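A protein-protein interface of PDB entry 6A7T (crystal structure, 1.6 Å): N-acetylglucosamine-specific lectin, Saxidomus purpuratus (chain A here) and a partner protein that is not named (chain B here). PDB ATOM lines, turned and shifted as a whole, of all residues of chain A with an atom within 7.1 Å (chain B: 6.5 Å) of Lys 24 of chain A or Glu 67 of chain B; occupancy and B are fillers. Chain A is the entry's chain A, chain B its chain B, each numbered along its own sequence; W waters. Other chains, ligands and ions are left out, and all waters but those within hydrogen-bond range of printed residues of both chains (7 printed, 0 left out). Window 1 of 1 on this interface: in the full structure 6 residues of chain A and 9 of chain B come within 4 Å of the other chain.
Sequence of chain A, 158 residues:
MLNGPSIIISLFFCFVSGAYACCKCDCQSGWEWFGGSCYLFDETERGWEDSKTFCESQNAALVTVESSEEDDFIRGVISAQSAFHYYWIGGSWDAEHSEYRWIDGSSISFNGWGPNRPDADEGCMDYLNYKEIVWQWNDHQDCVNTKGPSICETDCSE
SG of Cys 23 of chain A is disulfide-bonded to SG of Cys 68 of chain B, 2.1 Å away.
NZ of Lys 24 of chain A lies within salt-bridge range of OD2 of Asp 156 of chain B.
SG of Cys 25 of chain A is disulfide-bonded to SG of Cys 22 of chain B (2.1 Å).
The backbone carbonyl oxygen of Gly 36 of chain B lies close to the side-chain sulfur of Cys 25 of chain A (3.7 Å).
Water W5 lies within hydrogen-bond range of O of Glu 67 of chain B (2.5 Å), O of Cys 22 of chain A (2.9 Å) and OG1 of Thr 110 of chain B (3.2 Å).
Water W1 lies within hydrogen-bond range of OG of Ser 38 of chain B (2.6 Å), O of Gly 36 of chain B (3.3 Å) and SG of Cys 25 of chain A (3.6 Å).
Water W2 bridges the backbone carbonyl oxygen (O) of Asp 156 of chain B and the side-chain sulfur (SG) of Cys 25 of chain A.
Water W7 lies within hydrogen-bond range of N of Cys 25 of chain A, O of Gly 36 of chain B and N of Lys 24 of chain A.
Water W4 bridges the backbone NH of Lys 24 of chain A (3.1 Å) and the side-chain sulfur of Cys 68 of chain B (3.6 Å).
Water W6 bridges the side-chain hydroxyl of Ser 69 of chain B (3.1 Å) and the side-chain sulfur of Cys 23 of chain A (3.6 Å).
Of the 22 printed residues of chain B, 7 touch a printed residue of chain A.
Printed residues of chain B that touch a printed residue of chain A: Cys 22, Gly 36, Glu 67, Cys 68, Thr 110, Asp 156 and Ser 158.
Of the 11 printed residues of chain A, 4 touch a printed residue of chain B.
Printed residues of chain A that touch a printed residue of chain B: Cys 23, Lys 24, Cys 25 and Gly 36.
Among the printed residues, 8 pairs touch across the chains.
Among the printed residues, Asp or Glu carboxylates within 4 Å of a Lys or Arg side-chain nitrogen of the other chain: Lys 24 of chain A with Asp 156 of chain B.
The backbone NH (N) of Cys 23 of chain A is in hydrogen-bond range of the side-chain carboxylate (OD2) of Asp 26 of chain A (3.0 Å).
O of Cys 23 of chain A lies close to NE1 of Trp 33 of chain A (3.4 Å).
O of Asp 156 of chain B sits at hydrogen-bond distance from N of Cys 22 of chain B, at 3.2 Å.
OG1 of Thr 110 of chain B sits at hydrogen-bond distance from O of Glu 67 of chain B.
The side-chain carboxylate (OD1) of Asp 156 of chain B is in hydrogen-bond range of the side-chain hydroxyl (OG) of Ser 158 of chain B.
The side-chain sulfur (SG) of Cys 27 of chain A forms a disulfide with the side-chain sulfur (SG) of Cys 38 of chain A.
Among the printed residues, pairs that only touch across the chains: Lys 24 of chain A with Ser 158 of chain B (3.3 Å), Gly 36 of chain A with Thr 110 of chain B (3.8 Å), Lys 24 of chain A with Cys 22 of chain B (3.95 Å) and Lys 24 of chain A with Glu 67 of chain B (3.96 Å).
Of chain B, only Cys 22, Glu 67, Asp 156 and Ser 158 come within 4 Å of Lys 24 of chain A.
Printed residues of chain A within 4 Å of Gly 36 of chain B: Cys 25.
Of the printed residues of chain A, Asp 156 of chain B touches Lys 24.
Printed residues of chain A within 4 Å of Ser 158 of chain B: Lys 24.
The nearest residue of chain B that does not touch Lys 24 of chain A is Cys 68 of chain B (5.2 Å).
The nearest residue of chain A that does not touch Glu 67 of chain B is Trp 33 of chain A (4.03 Å).
The nearest printed residue of chain A that does not touch Cys 22 of chain B is Asp 26 of chain A (5.9 Å).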
ATOM      1  N   CYS A  22       4.911 -21.548  16.616  1.00  0.00           N
ATOM      2  CA  CYS A  22       5.208 -20.633  15.494  1.00  0.00           C
ATOM      3  C   CYS A  22       4.882 -21.287  14.140  1.00  0.00           C
ATOM      4  O   CYS A  22       5.309 -22.423  13.864  1.00  0.00           O
ATOM      5  CB  CYS A  22       6.683 -20.270  15.406  1.00  0.00           C
ATOM      6  SG  CYS A  22       7.284 -19.418  16.890  1.00  0.00           S
ATOM      7  N   CYS A  23       4.253 -20.505  13.251  1.00  0.00           N
ATOM      8  CA  CYS A  23       4.083 -20.896  11.875  1.00  0.00           C
ATOM      9  C   CYS A  23       5.455 -20.870  11.189  1.00  0.00           C
ATOM     10  O   CYS A  23       6.381 -20.167  11.582  1.00  0.00           O
ATOM     11  CB  CYS A  23       3.092 -20.013  11.115  1.00  0.00           C
ATOM     12  SG  CYS A  23       1.446 -19.886  11.881  1.00  0.00           S
ATOM     13  N   LYS A  24       5.604 -21.673  10.150  1.00  0.00           N
ATOM     14  CA  LYS A  24       6.873 -21.784   9.442  1.00  0.00           C
ATOM     15  C   LYS A  24       7.408 -20.446   8.901  1.00  0.00           C
ATOM     16  O   LYS A  24       8.627 -20.263   8.788  1.00  0.00           O
ATOM     17  CB  LYS A  24       6.709 -22.719   8.240  1.00  0.00           C
ATOM     18  CG  LYS A  24       6.712 -24.187   8.584  1.00  0.00           C
ATOM     19  CD  LYS A  24       6.766 -25.062   7.363  1.00  0.00           C
ATOM     20  CE  LYS A  24       8.067 -25.017   6.602  1.00  0.00           C
ATOM     21  NZ  LYS A  24       8.137 -26.165   5.664  1.00  0.00           N
ATOM     22  N   CYS A  25       6.525 -19.503   8.576  1.00  0.00           N
ATOM     23  CA  CYS A  25       6.937 -18.237   7.981  1.00  0.00           C
ATOM     24  C   CYS A  25       6.665 -17.081   8.934  1.00  0.00           C
ATOM     25  O   CYS A  25       6.633 -15.925   8.478  1.00  0.00           O
ATOM     26  CB  CYS A  25       6.224 -18.026   6.657  1.00  0.00           C
ATOM     27  SG  CYS A  25       6.645 -19.369   5.521  1.00  0.00           S
ATOM     28  N   ASP A  26       6.500 -17.404  10.223  1.00  0.00           N
ATOM     29  CA  ASP A  26       6.120 -16.427  11.281  1.00  0.00           C
ATOM     30  C   ASP A  26       7.360 -15.746  11.872  1.00  0.00           C
ATOM     31  O   ASP A  26       7.215 -14.795  12.624  1.00  0.00           O
ATOM     32  CB  ASP A  26       5.469 -17.084  12.507  1.00  0.00           C
ATOM     33  CG  ASP A  26       3.951 -17.086  12.587  1.00  0.00           C
ATOM     34  OD1 ASP A  26       3.325 -16.450  11.670  1.00  0.00           O
ATOM     35  OD2 ASP A  26       3.411 -17.642  13.652  1.00  0.00           O
ATOM     36  N   CYS A  27       8.553 -16.265  11.622  1.00  0.00           N
ATOM     37  CA  CYS A  27       9.724 -15.800  12.392  1.00  0.00           C
ATOM     38  C   CYS A  27      10.081 -14.353  12.012  1.00  0.00           C
ATOM     39  O   CYS A  27       9.937 -13.946  10.865  1.00  0.00           O
ATOM     40  CB  CYS A  27      10.919 -16.719  12.183  1.00  0.00           C
ATOM     41  SG  CYS A  27      10.692 -18.470  12.638  1.00  0.00           S
ATOM     42  N   GLU A  32      15.324 -18.134  12.529  1.00  0.00           N
ATOM     43  CA  GLU A  32      15.147 -19.362  11.743  1.00  0.00           C
ATOM     44  C   GLU A  32      14.110 -20.256  12.395  1.00  0.00           C
ATOM     45  O   GLU A  32      14.068 -20.384  13.577  1.00  0.00           O
ATOM     46  CB  GLU A  32      16.417 -20.201  11.735  1.00  0.00           C
ATOM     47  CG  GLU A  32      17.509 -19.640  10.887  1.00  0.00           C
ATOM     48  CD  GLU A  32      18.556 -20.739  10.757  1.00  0.00           C
ATOM     49  OE1 GLU A  32      19.731 -20.464  11.066  1.00  0.00           O
ATOM     50  OE2 GLU A  32      18.160 -21.891  10.361  1.00  0.00           O
ATOM     51  N   TRP A  33      13.309 -20.950  11.575  1.00  0.00           N
ATOM     52  CA  TRP A  33      12.284 -21.880  12.056  1.00  0.00           C
ATOM     53  C   TRP A  33      12.787 -23.323  12.045  1.00  0.00           C
ATOM     54  O   TRP A  33      13.426 -23.752  11.083  1.00  0.00           O
ATOM     55  CB  TRP A  33      11.047 -21.761  11.178  1.00  0.00           C
ATOM     56  CG  TRP A  33       9.849 -22.512  11.667  1.00  0.00           C
ATOM     57  CD1 TRP A  33       8.884 -22.003  12.483  1.00  0.00           C
ATOM     58  CD2 TRP A  33       9.472 -23.879  11.405  1.00  0.00           C
ATOM     59  NE1 TRP A  33       7.915 -22.937  12.686  1.00  0.00           N
ATOM     60  CE2 TRP A  33       8.238 -24.091  12.044  1.00  0.00           C
ATOM     61  CE3 TRP A  33      10.010 -24.913  10.627  1.00  0.00           C
ATOM     62  CZ2 TRP A  33       7.559 -25.309  12.027  1.00  0.00           C
ATOM     63  CZ3 TRP A  33       9.325 -26.122  10.585  1.00  0.00           C
ATOM     64  CH2 TRP A  33       8.135 -26.324  11.289  1.00  0.00           C
ATOM     65  N   PHE A  34      12.429 -24.046  13.089  1.00  0.00           N
ATOM     66  CA  PHE A  34      12.610 -25.478  13.141  1.00  0.00           C
ATOM     67  C   PHE A  34      11.643 -26.051  14.168  1.00  0.00           C
ATOM     68  O   PHE A  34      11.568 -25.574  15.279  1.00  0.00           O
ATOM     69  CB  PHE A  34      14.057 -25.823  13.505  1.00  0.00           C
ATOM     70  CG  PHE A  34      14.249 -27.302  13.712  1.00  0.00           C
ATOM     71  CD1 PHE A  34      14.352 -28.137  12.613  1.00  0.00           C
ATOM     72  CD2 PHE A  34      14.183 -27.856  14.977  1.00  0.00           C
ATOM     73  CE1 PHE A  34      14.448 -29.505  12.793  1.00  0.00           C
ATOM     74  CE2 PHE A  34      14.325 -29.223  15.151  1.00  0.00           C
ATOM     75  CZ  PHE A  34      14.450 -30.028  14.057  1.00  0.00           C
ATOM     76  N   GLY A  36       8.579 -26.150  15.069  1.00  0.00           N
ATOM     77  CA  GLY A  36       7.517 -25.395  15.671  1.00  0.00           C
ATOM     78  C   GLY A  36       8.000 -24.188  16.443  1.00  0.00           C
ATOM     79  O   GLY A  36       7.209 -23.478  17.060  1.00  0.00           O
ATOM     80  N   CYS A  38      10.822 -20.633  16.533  1.00  0.00           N
ATOM     81  CA  CYS A  38      11.751 -19.697  15.896  1.00  0.00           C
ATOM     82  C   CYS A  38      12.978 -19.501  16.806  1.00  0.00           C
ATOM     83  O   CYS A  38      12.865 -19.418  18.007  1.00  0.00           O
ATOM     84  CB  CYS A  38      11.082 -18.371  15.607  1.00  0.00           C
ATOM     85  SG  CYS A  38       9.711 -18.501  14.428  1.00  0.00           S
ATOM     86  N   CYS B  22       9.320 -20.417   2.220  1.00  0.00           N
ATOM     87  CA  CYS B  22       8.254 -19.381   2.301  1.00  0.00           C
ATOM     88  C   CYS B  22       7.995 -18.798   0.901  1.00  0.00           C
ATOM     89  O   CYS B  22       8.819 -18.086   0.330  1.00  0.00           O
ATOM     90  CB  CYS B  22       8.603 -18.335   3.356  1.00  0.00           C
ATOM     91  SG  CYS B  22       8.668 -19.034   5.030  1.00  0.00           S
ATOM     92  N   GLY B  36       0.074 -17.353   4.482  1.00  0.00           N
ATOM     93  CA  GLY B  36       1.200 -17.637   5.378  1.00  0.00           C
ATOM     94  C   GLY B  36       2.391 -18.345   4.727  1.00  0.00           C
ATOM     95  O   GLY B  36       2.952 -19.352   5.233  1.00  0.00           O
ATOM     96  N   SER B  38       2.582 -20.098   2.031  1.00  0.00           N
ATOM     97  CA  SER B  38       2.256 -21.325   1.333  1.00  0.00           C
ATOM     98  C   SER B  38       1.173 -21.069   0.287  1.00  0.00           C
ATOM     99  O   SER B  38       0.339 -20.183   0.382  1.00  0.00           O
ATOM    100  CB  SER B  38       1.776 -22.414   2.284  1.00  0.00           C
ATOM    101  OG  SER B  38       2.861 -23.017   2.980  1.00  0.00           O
ATOM    102  N   TYR B  40      -1.951 -23.216  -1.641  1.00  0.00           N
ATOM    103  CA  TYR B  40      -2.825 -24.350  -1.331  1.00  0.00           C
ATOM    104  C   TYR B  40      -3.775 -24.647  -2.501  1.00  0.00           C
ATOM    105  O   TYR B  40      -4.378 -23.714  -3.097  1.00  0.00           O
ATOM    106  CB  TYR B  40      -3.671 -24.061  -0.089  1.00  0.00           C
ATOM    107  CG  TYR B  40      -2.889 -23.778   1.165  1.00  0.00           C
ATOM    108  CD1 TYR B  40      -2.402 -22.510   1.470  1.00  0.00           C
ATOM    109  CD2 TYR B  40      -2.586 -24.792   2.046  1.00  0.00           C
ATOM    110  CE1 TYR B  40      -1.672 -22.250   2.615  1.00  0.00           C
ATOM    111  CE2 TYR B  40      -1.843 -24.558   3.198  1.00  0.00           C
ATOM    112  CZ  TYR B  40      -1.380 -23.282   3.487  1.00  0.00           C
ATOM    113  OH  TYR B  40      -0.650 -23.051   4.619  1.00  0.00           O
ATOM    114  N   VAL B  64      -1.246 -31.324   2.426  1.00  0.00           N
ATOM    115  CA  VAL B  64      -0.972 -30.226   3.340  1.00  0.00           C
ATOM    116  C   VAL B  64      -0.516 -30.771   4.686  1.00  0.00           C
ATOM    117  O   VAL B  64      -0.986 -31.841   5.163  1.00  0.00           O
ATOM    118  CB  VAL B  64      -2.206 -29.329   3.462  1.00  0.00           C
ATOM    119  CG1 VAL B  64      -3.370 -30.095   4.038  1.00  0.00           C
ATOM    120  CG2 VAL B  64      -1.942 -28.108   4.310  1.00  0.00           C
ATOM    121  N   THR B  65       0.466 -30.049   5.286  1.00  0.00           N
ATOM    122  CA  THR B  65       0.945 -30.284   6.637  1.00  0.00           C
ATOM    123  C   THR B  65       0.629 -29.015   7.422  1.00  0.00           C
ATOM    124  O   THR B  65       0.786 -27.917   6.877  1.00  0.00           O
ATOM    125  CB  THR B  65       2.433 -30.690   6.657  1.00  0.00           C
ATOM    126  OG1 THR B  65       3.237 -29.602   6.201  1.00  0.00           O
ATOM    127  CG2 THR B  65       2.719 -31.913   5.829  1.00  0.00           C
ATOM    128  N   VAL B  66       0.153 -29.158   8.643  1.00  0.00           N
ATOM    129  CA  VAL B  66      -0.406 -28.013   9.359  1.00  0.00           C
ATOM    130  C   VAL B  66       0.421 -27.754  10.627  1.00  0.00           C
ATOM    131  O   VAL B  66       0.306 -28.515  11.611  1.00  0.00           O
ATOM    132  CB  VAL B  66      -1.886 -28.273   9.691  1.00  0.00           C
ATOM    133  CG1 VAL B  66      -2.546 -27.125  10.430  1.00  0.00           C
ATOM    134  CG2 VAL B  66      -2.691 -28.639   8.438  1.00  0.00           C
ATOM    135  N   GLU B  67       1.286 -26.722  10.568  1.00  0.00           N
ATOM    136  CA  GLU B  67       2.317 -26.519  11.594  1.00  0.00           C
ATOM    137  C   GLU B  67       1.818 -25.602  12.701  1.00  0.00           C
ATOM    138  O   GLU B  67       2.448 -25.579  13.744  1.00  0.00           O
ATOM    139  CB  GLU B  67       3.598 -25.989  10.954  1.00  0.00           C
ATOM    140  CG  GLU B  67       4.320 -27.072  10.219  1.00  0.00           C
ATOM    141  CD  GLU B  67       3.832 -27.358   8.809  1.00  0.00           C
ATOM    142  OE1 GLU B  67       3.164 -26.455   8.233  1.00  0.00           O
ATOM    143  OE2 GLU B  67       4.305 -28.379   8.251  1.00  0.00           O
ATOM    144  N   CYS B  68       0.714 -24.885  12.502  1.00  0.00           N
ATOM    145  CA  CYS B  68       0.285 -23.922  13.502  1.00  0.00           C
ATOM    146  C   CYS B  68      -1.204 -23.670  13.442  1.00  0.00           C
ATOM    147  O   CYS B  68      -1.897 -23.975  12.422  1.00  0.00           O
ATOM    148  CB  CYS B  68       1.000 -22.583  13.335  1.00  0.00           C
ATOM    149  SG  CYS B  68       0.656 -21.777  11.742  1.00  0.00           S
ATOM    150  N   SER B  69      -1.701 -23.042  14.507  1.00  0.00           N
ATOM    151  CA  SER B  69      -3.134 -22.742  14.634  1.00  0.00           C
ATOM    152  C   SER B  69      -3.629 -21.731  13.592  1.00  0.00           C
ATOM    153  O   SER B  69      -4.758 -21.848  13.090  1.00  0.00           O
ATOM    154  CB  SER B  69      -3.437 -22.330  16.051  1.00  0.00           C
ATOM    155  OG  SER B  69      -2.975 -21.005  16.272  1.00  0.00           O
ATOM    156  N   GLU B  71      -2.645 -21.569  10.447  1.00  0.00           N
ATOM    157  CA  GLU B  71      -2.795 -22.300   9.196  1.00  0.00           C
ATOM    158  C   GLU B  71      -4.067 -23.173   9.309  1.00  0.00           C
ATOM    159  O   GLU B  71      -4.842 -23.268   8.396  1.00  0.00           O
ATOM    160  CB  GLU B  71      -1.545 -23.149   8.972  1.00  0.00           C
ATOM    161  CG  GLU B  71      -1.535 -23.877   7.651  1.00  0.00           C
ATOM    162  CD  GLU B  71      -0.270 -24.633   7.353  1.00  0.00           C
ATOM    163  OE1 GLU B  71       0.558 -24.923   8.283  1.00  0.00           O
ATOM    164  OE2 GLU B  71      -0.124 -25.002   6.205  1.00  0.00           O
ATOM    165  N   ASP B  72      -4.225 -23.817  10.462  1.00  0.00           N
ATOM    166  CA  ASP B  72      -5.422 -24.607  10.761  1.00  0.00           C
ATOM    167  C   ASP B  72      -6.648 -23.706  10.592  1.00  0.00           C
ATOM    168  O   ASP B  72      -7.630 -24.113   9.991  1.00  0.00           O
ATOM    169  CB  ASP B  72      -5.369 -25.166  12.179  1.00  0.00           C
ATOM    170  CG  ASP B  72      -6.582 -25.986  12.579  1.00  0.00           C
ATOM    171  OD1 ASP B  72      -6.692 -27.099  12.071  1.00  0.00           O
ATOM    172  OD2 ASP B  72      -7.331 -25.541  13.465  1.00  0.00           O
ATOM    173  N   TRP B 103       3.347 -36.164  10.022  1.00  0.00           N
ATOM    174  CA  TRP B 103       3.272 -35.694   8.696  1.00  0.00           C
ATOM    175  C   TRP B 103       4.082 -36.604   7.782  1.00  0.00           C
ATOM    176  O   TRP B 103       5.013 -37.246   8.235  1.00  0.00           O
ATOM    177  CB  TRP B 103       3.717 -34.233   8.572  1.00  0.00           C
ATOM    178  CG  TRP B 103       2.947 -33.327   9.479  1.00  0.00           C
ATOM    179  CD1 TRP B 103       3.432 -32.603  10.530  1.00  0.00           C
ATOM    180  CD2 TRP B 103       1.544 -33.001   9.405  1.00  0.00           C
ATOM    181  NE1 TRP B 103       2.429 -31.875  11.131  1.00  0.00           N
ATOM    182  CE2 TRP B 103       1.252 -32.117  10.456  1.00  0.00           C
ATOM    183  CE3 TRP B 103       0.502 -33.410   8.565  1.00  0.00           C
ATOM    184  CZ2 TRP B 103      -0.026 -31.633  10.722  1.00  0.00           C
ATOM    185  CZ3 TRP B 103      -0.752 -32.906   8.810  1.00  0.00           C
ATOM    186  CH2 TRP B 103      -1.022 -32.055   9.867  1.00  0.00           C
ATOM    187  N   ASP B 105       6.229 -36.077   5.622  1.00  0.00           N
ATOM    188  CA  ASP B 105       7.634 -35.699   5.476  1.00  0.00           C
ATOM    189  C   ASP B 105       8.451 -36.284   6.619  1.00  0.00           C
ATOM    190  O   ASP B 105       9.648 -36.053   6.669  1.00  0.00           O
ATOM    191  CB  ASP B 105       7.822 -34.189   5.395  1.00  0.00           C
ATOM    192  CG  ASP B 105       7.447 -33.382   6.643  1.00  0.00           C
ATOM    193  OD1 ASP B 105       6.809 -33.928   7.545  1.00  0.00           O
ATOM    194  OD2 ASP B 105       7.756 -32.161   6.657  1.00  0.00           O
ATOM    195  N   SER B 107       8.019 -35.357   9.769  1.00  0.00           N
ATOM    196  CA  SER B 107       8.049 -34.400  10.861  1.00  0.00           C
ATOM    197  C   SER B 107       6.938 -34.710  11.854  1.00  0.00           C
ATOM    198  O   SER B 107       5.800 -34.952  11.451  1.00  0.00           O
ATOM    199  CB  SER B 107       7.998 -32.992  10.395  1.00  0.00           C
ATOM    200  OG  SER B 107       6.779 -32.674   9.770  1.00  0.00           O
ATOM    201  N   THR B 110       3.366 -30.567  15.535  1.00  0.00           N
ATOM    202  CA  THR B 110       3.600 -29.440  16.404  1.00  0.00           C
ATOM    203  C   THR B 110       2.252 -28.992  16.940  1.00  0.00           C
ATOM    204  O   THR B 110       1.858 -29.316  18.045  1.00  0.00           O
ATOM    205  CB  THR B 110       4.405 -28.362  15.661  1.00  0.00           C
ATOM    206  OG1 THR B 110       3.906 -28.094  14.346  1.00  0.00           O
ATOM    207  CG2 THR B 110       5.847 -28.770  15.466  1.00  0.00           C
ATOM    208  N   PHE B 111       1.503 -28.257  16.116  1.00  0.00           N
ATOM    209  CA  PHE B 111       0.105 -27.992  16.368  1.00  0.00           C
ATOM    210  C   PHE B 111      -0.647 -29.326  16.350  1.00  0.00           C
ATOM    211  O   PHE B 111      -0.297 -30.172  15.562  1.00  0.00           O
ATOM    212  CB  PHE B 111      -0.445 -27.070  15.278  1.00  0.00           C
ATOM    213  CG  PHE B 111      -1.945 -26.910  15.303  1.00  0.00           C
ATOM    214  CD1 PHE B 111      -2.564 -26.102  16.232  1.00  0.00           C
ATOM    215  CD2 PHE B 111      -2.757 -27.613  14.417  1.00  0.00           C
ATOM    216  CE1 PHE B 111      -3.950 -25.987  16.282  1.00  0.00           C
ATOM    217  CE2 PHE B 111      -4.134 -27.517  14.486  1.00  0.00           C
ATOM    218  CZ  PHE B 111      -4.739 -26.682  15.385  1.00  0.00           C
ATOM    219  N   GLU B 154      -0.375 -28.547  -0.837  1.00  0.00           N
ATOM    220  CA  GLU B 154       0.406 -27.402  -0.300  1.00  0.00           C
ATOM    221  C   GLU B 154       1.760 -27.352  -1.016  1.00  0.00           C
ATOM    222  O   GLU B 154       2.414 -28.341  -1.128  1.00  0.00           O
ATOM    223  CB  GLU B 154       0.633 -27.547   1.203  1.00  0.00           C
ATOM    224  CG  GLU B 154       1.326 -26.327   1.817  1.00  0.00           C
ATOM    225  CD  GLU B 154       1.619 -26.394   3.310  1.00  0.00           C
ATOM    226  OE1 GLU B 154       1.487 -27.522   3.893  1.00  0.00           O
ATOM    227  OE2 GLU B 154       2.016 -25.349   3.888  1.00  0.00           O
ATOM    228  N   ASP B 156       5.100 -25.112  -0.144  1.00  0.00           N
ATOM    229  CA  ASP B 156       5.561 -24.223   0.935  1.00  0.00           C
ATOM    230  C   ASP B 156       6.952 -23.647   0.636  1.00  0.00           C
ATOM    231  O   ASP B 156       7.402 -22.823   1.414  1.00  0.00           O
ATOM    232  CB  ASP B 156       5.483 -24.876   2.323  1.00  0.00           C
ATOM    233  CG  ASP B 156       6.433 -26.017   2.568  1.00  0.00           C
ATOM    234  OD1 ASP B 156       7.288 -26.245   1.708  1.00  0.00           O
ATOM    235  OD2 ASP B 156       6.282 -26.712   3.610  1.00  0.00           O
ATOM    236  N   CYS B 157       7.542 -23.973  -0.522  1.00  0.00           N
ATOM    237  CA  CYS B 157       8.823 -23.376  -0.962  1.00  0.00           C
ATOM    238  C   CYS B 157       9.869 -23.476   0.163  1.00  0.00           C
ATOM    239  O   CYS B 157      10.686 -22.551   0.356  1.00  0.00           O
ATOM    240  CB  CYS B 157       8.639 -21.920  -1.380  1.00  0.00           C
ATOM    241  SG  CYS B 157       7.381 -21.596  -2.653  1.00  0.00           S
ATOM    242  N   SER B 158       9.833 -24.576   0.929  1.00  0.00           N
ATOM    243  CA  SER B 158      10.798 -24.825   1.993  1.00  0.00           C
ATOM    244  C   SER B 158      12.050 -25.497   1.408  1.00  0.00           C
ATOM    245  O   SER B 158      12.092 -25.817   0.223  1.00  0.00           O
ATOM    246  CB  SER B 158      10.180 -25.637   3.116  1.00  0.00           C
ATOM    247  OG  SER B 158       9.821 -26.946   2.685  1.00  0.00           O
ATOM    248  N   ASP B 159      13.065 -25.694   2.260  1.00  0.00           N
ATOM    249  CA  ASP B 159      14.372 -26.233   1.867  1.00  0.00           C
ATOM    250  C   ASP B 159      14.196 -27.690   1.414  1.00  0.00           C
ATOM    251  O   ASP B 159      15.156 -28.355   1.006  1.00  0.00           O
ATOM    252  CB  ASP B 159      15.399 -26.075   3.001  1.00  0.00           C
ATOM    253  CG  ASP B 159      15.542 -27.265   3.950  1.00  0.00           C
ATOM    254  OD1 ASP B 159      16.218 -28.246   3.565  1.00  0.00           O
ATOM    255  OD2 ASP B 159      14.998 -27.198   5.079  1.00  0.00           O
HETATM  256  O   HOH W   1       4.591 -22.180   4.801  1.00  0.00           O
HETATM  257  O   HOH W   2       7.113 -22.528   4.141  1.00  0.00           O
HETATM  258  O   HOH W   3       0.914 -20.420   8.522  1.00  0.00           O
HETATM  259  O   HOH W   4       2.979 -22.961   9.278  1.00  0.00           O
HETATM  260  O   HOH W   5       4.609 -25.007  14.892  1.00  0.00           O
HETATM  261  O   HOH W   6      -0.520 -19.841  14.877  1.00  0.00           O
HETATM  262  O   HOH W   7       3.652 -20.027   8.048  1.00  0.00           O
